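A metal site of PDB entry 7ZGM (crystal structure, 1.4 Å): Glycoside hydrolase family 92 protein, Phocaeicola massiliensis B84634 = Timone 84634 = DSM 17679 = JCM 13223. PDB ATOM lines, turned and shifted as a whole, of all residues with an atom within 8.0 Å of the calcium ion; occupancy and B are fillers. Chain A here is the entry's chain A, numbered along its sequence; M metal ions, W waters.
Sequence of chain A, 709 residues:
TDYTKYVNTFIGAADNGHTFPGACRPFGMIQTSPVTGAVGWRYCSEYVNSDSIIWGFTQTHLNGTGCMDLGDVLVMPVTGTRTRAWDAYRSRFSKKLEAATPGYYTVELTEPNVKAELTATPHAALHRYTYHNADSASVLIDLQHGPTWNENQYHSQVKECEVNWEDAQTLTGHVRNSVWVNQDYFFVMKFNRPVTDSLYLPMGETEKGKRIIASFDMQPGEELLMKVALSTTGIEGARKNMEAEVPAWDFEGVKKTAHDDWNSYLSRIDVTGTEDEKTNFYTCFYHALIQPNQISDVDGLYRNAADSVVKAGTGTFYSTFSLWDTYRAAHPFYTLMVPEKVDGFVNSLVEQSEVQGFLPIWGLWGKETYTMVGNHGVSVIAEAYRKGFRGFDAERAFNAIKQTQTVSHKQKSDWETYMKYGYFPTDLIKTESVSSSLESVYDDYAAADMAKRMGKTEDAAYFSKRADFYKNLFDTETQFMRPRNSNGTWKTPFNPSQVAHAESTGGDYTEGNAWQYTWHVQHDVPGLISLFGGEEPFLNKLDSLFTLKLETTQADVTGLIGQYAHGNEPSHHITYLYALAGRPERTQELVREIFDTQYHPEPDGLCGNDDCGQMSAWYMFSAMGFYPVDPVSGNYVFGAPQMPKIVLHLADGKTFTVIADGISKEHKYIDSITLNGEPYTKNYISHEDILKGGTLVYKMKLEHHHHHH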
ATOM      1  N   GLY A  64     -17.432 -29.254 -15.602  1.00  0.00           N
ATOM      2  CA  GLY A  64     -16.474 -28.282 -16.092  1.00  0.00           C
ATOM      3  C   GLY A  64     -16.956 -26.836 -16.073  1.00  0.00           C
ATOM      4  O   GLY A  64     -16.399 -26.002 -16.787  1.00  0.00           O
ATOM      5  N   THR A  65     -17.992 -26.528 -15.280  1.00  0.00           N
ATOM      6  CA  THR A  65     -18.479 -25.180 -15.116  1.00  0.00           C
ATOM      7  C   THR A  65     -17.505 -24.396 -14.241  1.00  0.00           C
ATOM      8  O   THR A  65     -16.751 -24.978 -13.451  1.00  0.00           O
ATOM      9  CB  THR A  65     -19.874 -25.184 -14.488  1.00  0.00           C
ATOM     10  OG1 THR A  65     -19.742 -25.952 -13.294  1.00  0.00           O
ATOM     11  CG2 THR A  65     -20.948 -25.768 -15.377  1.00  0.00           C
ATOM     12  N   GLY A  66     -17.576 -23.072 -14.335  1.00  0.00           N
ATOM     13  CA  GLY A  66     -16.799 -22.191 -13.484  1.00  0.00           C
ATOM     14  C   GLY A  66     -17.158 -22.369 -12.007  1.00  0.00           C
ATOM     15  O   GLY A  66     -16.269 -22.562 -11.187  1.00  0.00           O
ATOM     16  N   TRP A 324     -22.851 -20.103 -24.349  1.00  0.00           N
ATOM     17  CA  TRP A 324     -21.722 -19.220 -24.635  1.00  0.00           C
ATOM     18  C   TRP A 324     -20.493 -20.033 -25.028  1.00  0.00           C
ATOM     19  O   TRP A 324     -19.743 -19.616 -25.907  1.00  0.00           O
ATOM     20  CB  TRP A 324     -21.411 -18.338 -23.434  1.00  0.00           C
ATOM     21  CG  TRP A 324     -20.277 -17.385 -23.658  1.00  0.00           C
ATOM     22  CD1 TRP A 324     -20.302 -16.211 -24.348  1.00  0.00           C
ATOM     23  CD2 TRP A 324     -18.934 -17.520 -23.149  1.00  0.00           C
ATOM     24  NE1 TRP A 324     -19.073 -15.591 -24.286  1.00  0.00           N
ATOM     25  CE2 TRP A 324     -18.224 -16.365 -23.546  1.00  0.00           C
ATOM     26  CE3 TRP A 324     -18.279 -18.474 -22.355  1.00  0.00           C
ATOM     27  CZ2 TRP A 324     -16.900 -16.153 -23.195  1.00  0.00           C
ATOM     28  CZ3 TRP A 324     -16.961 -18.265 -22.017  1.00  0.00           C
ATOM     29  CH2 TRP A 324     -16.276 -17.118 -22.440  1.00  0.00           C
ATOM     30  N   ASP A 325     -20.277 -21.178 -24.364  1.00  0.00           N
ATOM     31  CA  ASP A 325     -19.182 -22.064 -24.692  1.00  0.00           C
ATOM     32  C   ASP A 325     -19.513 -22.965 -25.881  1.00  0.00           C
ATOM     33  O   ASP A 325     -18.733 -23.079 -26.828  1.00  0.00           O
ATOM     34  CB  ASP A 325     -18.834 -22.955 -23.502  1.00  0.00           C
ATOM     35  CG  ASP A 325     -18.639 -22.171 -22.222  1.00  0.00           C
ATOM     36  OD1 ASP A 325     -17.524 -21.679 -22.012  1.00  0.00           O
ATOM     37  OD2 ASP A 325     -19.630 -22.012 -21.488  1.00  0.00           O
ATOM     38  N   MET A 372     -22.887 -15.436 -18.775  1.00  0.00           N
ATOM     39  CA  MET A 372     -22.049 -15.027 -19.902  1.00  0.00           C
ATOM     40  C   MET A 372     -22.818 -14.049 -20.799  1.00  0.00           C
ATOM     41  O   MET A 372     -23.610 -13.262 -20.297  1.00  0.00           O
ATOM     42  CB  MET A 372     -21.499 -16.219 -20.692  1.00  0.00           C
ATOM     43  CG  MET A 372     -20.935 -17.325 -19.820  1.00  0.00           C
ATOM     44  SD  MET A 372     -19.824 -16.747 -18.530  1.00  0.00           S
ATOM     45  CE  MET A 372     -18.572 -16.033 -19.557  1.00  0.00           C
ATOM     46  N   GLU A 511     -14.251 -12.235 -19.526  1.00  0.00           N
ATOM     47  CA  GLU A 511     -13.266 -13.201 -19.047  1.00  0.00           C
ATOM     48  C   GLU A 511     -11.963 -13.076 -19.835  1.00  0.00           C
ATOM     49  O   GLU A 511     -11.156 -14.013 -19.878  1.00  0.00           O
ATOM     50  CB  GLU A 511     -13.806 -14.628 -19.133  1.00  0.00           C
ATOM     51  CG  GLU A 511     -15.072 -14.849 -18.318  1.00  0.00           C
ATOM     52  CD  GLU A 511     -14.911 -14.523 -16.844  1.00  0.00           C
ATOM     53  OE1 GLU A 511     -14.038 -15.123 -16.203  1.00  0.00           O
ATOM     54  OE2 GLU A 511     -15.654 -13.644 -16.346  1.00  0.00           O
ATOM     55  N   ALA A 565      -5.507 -17.201 -24.961  1.00  0.00           N
ATOM     56  CA  ALA A 565      -5.885 -17.907 -23.746  1.00  0.00           C
ATOM     57  C   ALA A 565      -6.730 -19.121 -24.112  1.00  0.00           C
ATOM     58  O   ALA A 565      -7.927 -18.987 -24.395  1.00  0.00           O
ATOM     59  CB  ALA A 565      -6.638 -16.983 -22.838  1.00  0.00           C
ATOM     60  N   HIS A 566      -6.124 -20.311 -24.105  1.00  0.00           N
ATOM     61  CA  HIS A 566      -6.809 -21.475 -24.646  1.00  0.00           C
ATOM     62  C   HIS A 566      -8.061 -21.843 -23.843  1.00  0.00           C
ATOM     63  O   HIS A 566      -9.005 -22.371 -24.423  1.00  0.00           O
ATOM     64  CB  HIS A 566      -5.873 -22.688 -24.791  1.00  0.00           C
ATOM     65  CG  HIS A 566      -6.515 -23.775 -25.587  1.00  0.00           C
ATOM     66  ND1 HIS A 566      -6.910 -23.616 -26.900  1.00  0.00           N
ATOM     67  CD2 HIS A 566      -6.969 -25.003 -25.177  1.00  0.00           C
ATOM     68  CE1 HIS A 566      -7.560 -24.713 -27.274  1.00  0.00           C
ATOM     69  NE2 HIS A 566      -7.594 -25.587 -26.240  1.00  0.00           N
ATOM     70  N   GLY A 567      -8.076 -21.535 -22.530  1.00  0.00           N
ATOM     71  CA  GLY A 567      -9.223 -21.823 -21.667  1.00  0.00           C
ATOM     72  C   GLY A 567     -10.398 -20.837 -21.779  1.00  0.00           C
ATOM     73  O   GLY A 567     -11.486 -21.049 -21.194  1.00  0.00           O
ATOM     74  N   ASN A 568     -10.172 -19.754 -22.536  1.00  0.00           N
ATOM     75  CA  ASN A 568     -11.200 -18.751 -22.755  1.00  0.00           C
ATOM     76  C   ASN A 568     -11.751 -18.929 -24.164  1.00  0.00           C
ATOM     77  O   ASN A 568     -11.066 -18.707 -25.167  1.00  0.00           O
ATOM     78  CB  ASN A 568     -10.689 -17.330 -22.517  1.00  0.00           C
ATOM     79  CG  ASN A 568     -11.818 -16.333 -22.326  1.00  0.00           C
ATOM     80  OD1 ASN A 568     -12.822 -16.637 -21.664  1.00  0.00           O
ATOM     81  ND2 ASN A 568     -11.677 -15.157 -22.912  1.00  0.00           N
ATOM     82  N   GLU A 569     -13.043 -19.256 -24.208  1.00  0.00           N
ATOM     83  CA  GLU A 569     -13.702 -19.690 -25.418  1.00  0.00           C
ATOM     84  C   GLU A 569     -13.606 -18.685 -26.559  1.00  0.00           C
ATOM     85  O   GLU A 569     -13.527 -19.118 -27.714  1.00  0.00           O
ATOM     86  CB  GLU A 569     -15.158 -20.051 -25.094  1.00  0.00           C
ATOM     87  CG  GLU A 569     -15.305 -21.477 -24.625  1.00  0.00           C
ATOM     88  CD  GLU A 569     -14.771 -21.832 -23.238  1.00  0.00           C
ATOM     89  OE1 GLU A 569     -14.414 -20.930 -22.391  1.00  0.00           O
ATOM     90  OE2 GLU A 569     -14.748 -23.058 -22.983  1.00  0.00           O
ATOM     91  N   PRO A 570     -13.653 -17.352 -26.338  1.00  0.00           N
ATOM     92  CA  PRO A 570     -13.426 -16.379 -27.406  1.00  0.00           C
ATOM     93  C   PRO A 570     -12.163 -16.616 -28.228  1.00  0.00           C
ATOM     94  O   PRO A 570     -12.106 -16.219 -29.395  1.00  0.00           O
ATOM     95  CB  PRO A 570     -13.366 -15.055 -26.643  1.00  0.00           C
ATOM     96  CG  PRO A 570     -14.341 -15.262 -25.512  1.00  0.00           C
ATOM     97  CD  PRO A 570     -14.060 -16.695 -25.077  1.00  0.00           C
ATOM     98  N   HIS A 572     -11.010 -19.641 -29.038  1.00  0.00           N
ATOM     99  CA  HIS A 572     -10.928 -20.985 -29.585  1.00  0.00           C
ATOM    100  C   HIS A 572     -10.752 -21.046 -31.104  1.00  0.00           C
ATOM    101  O   HIS A 572     -10.124 -21.968 -31.601  1.00  0.00           O
ATOM    102  CB  HIS A 572     -12.143 -21.826 -29.179  1.00  0.00           C
ATOM    103  CG  HIS A 572     -12.030 -22.387 -27.807  1.00  0.00           C
ATOM    104  ND1 HIS A 572     -12.955 -23.212 -27.239  1.00  0.00           N
ATOM    105  CD2 HIS A 572     -11.031 -22.186 -26.898  1.00  0.00           C
ATOM    106  CE1 HIS A 572     -12.552 -23.545 -26.027  1.00  0.00           C
ATOM    107  NE2 HIS A 572     -11.364 -22.911 -25.780  1.00  0.00           N
ATOM    108  N   GLY A 608      -7.682 -25.769 -18.296  1.00  0.00           N
ATOM    109  CA  GLY A 608      -8.855 -25.015 -17.932  1.00  0.00           C
ATOM    110  C   GLY A 608     -10.066 -25.920 -17.769  1.00  0.00           C
ATOM    111  O   GLY A 608     -10.025 -27.100 -18.118  1.00  0.00           O
ATOM    112  N   ASN A 609     -11.131 -25.337 -17.250  1.00  0.00           N
ATOM    113  CA  ASN A 609     -12.381 -26.047 -17.042  1.00  0.00           C
ATOM    114  C   ASN A 609     -12.907 -26.580 -18.364  1.00  0.00           C
ATOM    115  O   ASN A 609     -12.811 -25.894 -19.376  1.00  0.00           O
ATOM    116  CB  ASN A 609     -13.394 -25.128 -16.352  1.00  0.00           C
ATOM    117  CG  ASN A 609     -12.922 -24.658 -14.996  1.00  0.00           C
ATOM    118  OD1 ASN A 609     -12.119 -25.312 -14.350  1.00  0.00           O
ATOM    119  ND2 ASN A 609     -13.429 -23.509 -14.585  1.00  0.00           N
ATOM    120  N   ASP A 610     -13.511 -27.772 -18.338  1.00  0.00           N
ATOM    121  CA  ASP A 610     -13.977 -28.394 -19.566  1.00  0.00           C
ATOM    122  C   ASP A 610     -15.116 -27.598 -20.212  1.00  0.00           C
ATOM    123  O   ASP A 610     -15.350 -27.715 -21.426  1.00  0.00           O
ATOM    124  CB  ASP A 610     -14.395 -29.841 -19.329  1.00  0.00           C
ATOM    125  CG  ASP A 610     -14.733 -30.546 -20.631  1.00  0.00           C
ATOM    126  OD1 ASP A 610     -13.853 -30.594 -21.521  1.00  0.00           O
ATOM    127  OD2 ASP A 610     -15.884 -31.021 -20.756  1.00  0.00           O
ATOM    128  N   ASP A 611     -15.877 -26.828 -19.424  1.00  0.00           N
ATOM    129  CA  ASP A 611     -16.897 -25.930 -19.959  1.00  0.00           C
ATOM    130  C   ASP A 611     -17.974 -26.746 -20.690  1.00  0.00           C
ATOM    131  O   ASP A 611     -18.297 -26.478 -21.837  1.00  0.00           O
ATOM    132  CB  ASP A 611     -16.234 -24.810 -20.789  1.00  0.00           C
ATOM    133  CG  ASP A 611     -15.269 -23.912 -20.008  1.00  0.00           C
ATOM    134  OD1 ASP A 611     -15.292 -23.970 -18.759  1.00  0.00           O
ATOM    135  OD2 ASP A 611     -14.472 -23.162 -20.618  1.00  0.00           O
ATOM    136  N   GLN A 614     -17.067 -28.163 -24.144  1.00  0.00           N
ATOM    137  CA  GLN A 614     -16.527 -27.325 -25.211  1.00  0.00           C
ATOM    138  C   GLN A 614     -15.024 -27.505 -25.368  1.00  0.00           C
ATOM    139  O   GLN A 614     -14.525 -27.565 -26.497  1.00  0.00           O
ATOM    140  CB  GLN A 614     -16.881 -25.851 -24.996  1.00  0.00           C
ATOM    141  CG  GLN A 614     -16.159 -24.904 -25.943  1.00  0.00           C
ATOM    142  CD  GLN A 614     -16.383 -25.163 -27.409  1.00  0.00           C
ATOM    143  OE1 GLN A 614     -17.377 -25.776 -27.825  1.00  0.00           O
ATOM    144  NE2 GLN A 614     -15.477 -24.631 -28.221  1.00  0.00           N
ATOM    145  N   MET A 615     -14.276 -27.563 -24.264  1.00  0.00           N
ATOM    146  CA  MET A 615     -12.842 -27.773 -24.381  1.00  0.00           C
ATOM    147  C   MET A 615     -12.536 -29.133 -25.016  1.00  0.00           C
ATOM    148  O   MET A 615     -11.567 -29.283 -25.749  1.00  0.00           O
ATOM    149  CB  MET A 615     -12.158 -27.679 -23.017  1.00  0.00           C
ATOM    150  CG  MET A 615     -12.244 -26.295 -22.397  1.00  0.00           C
ATOM    151  SD  MET A 615     -11.286 -25.015 -23.253  1.00  0.00           S
ATOM    152  CE  MET A 615      -9.623 -25.584 -22.933  1.00  0.00           C
HETATM  153 CA    CA M   1     -13.651 -20.997 -20.115  1.00  0.00          CA
HETATM  154  O   HOH W   1     -11.539 -23.533 -19.974  1.00  0.00           O
HETATM  155  O   HOH W   2     -13.420 -18.367 -19.733  1.00  0.00           O
HETATM  156  O   HOH W   3     -16.678 -20.877 -19.679  1.00  0.00           O
HETATM  157  O   HOH W   4     -13.290 -21.770 -18.133  1.00  0.00           O
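The calcium ion is bound by water W4 (2.2 Å), the side-chain carboxylate (OD2) of Asp 611 (2.4 Å), the side-chain carboxylate (OE1) of Glu 569 (2.4 Å), the backbone carbonyl oxygen (O) of Gly 567 (2.4 Å) and water W2 (2.7 Å). Slightly farther from the calcium ion lies water W3 (3.1 Å).
Three residues have an atom within 4 Å of the calcium ion: Gly 567, Glu 569 and Asp 611. The nearest printed residue that does not touch the calcium ion is Asn 568 (4.2 Å).
Water W1 lies within hydrogen-bond range of the backbone carbonyl oxygen of Asn 609 and the side-chain sulfur of Met 615.
N of Asp 611 is in hydrogen-bond range of O of Gly 64, 2.8 Å away.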
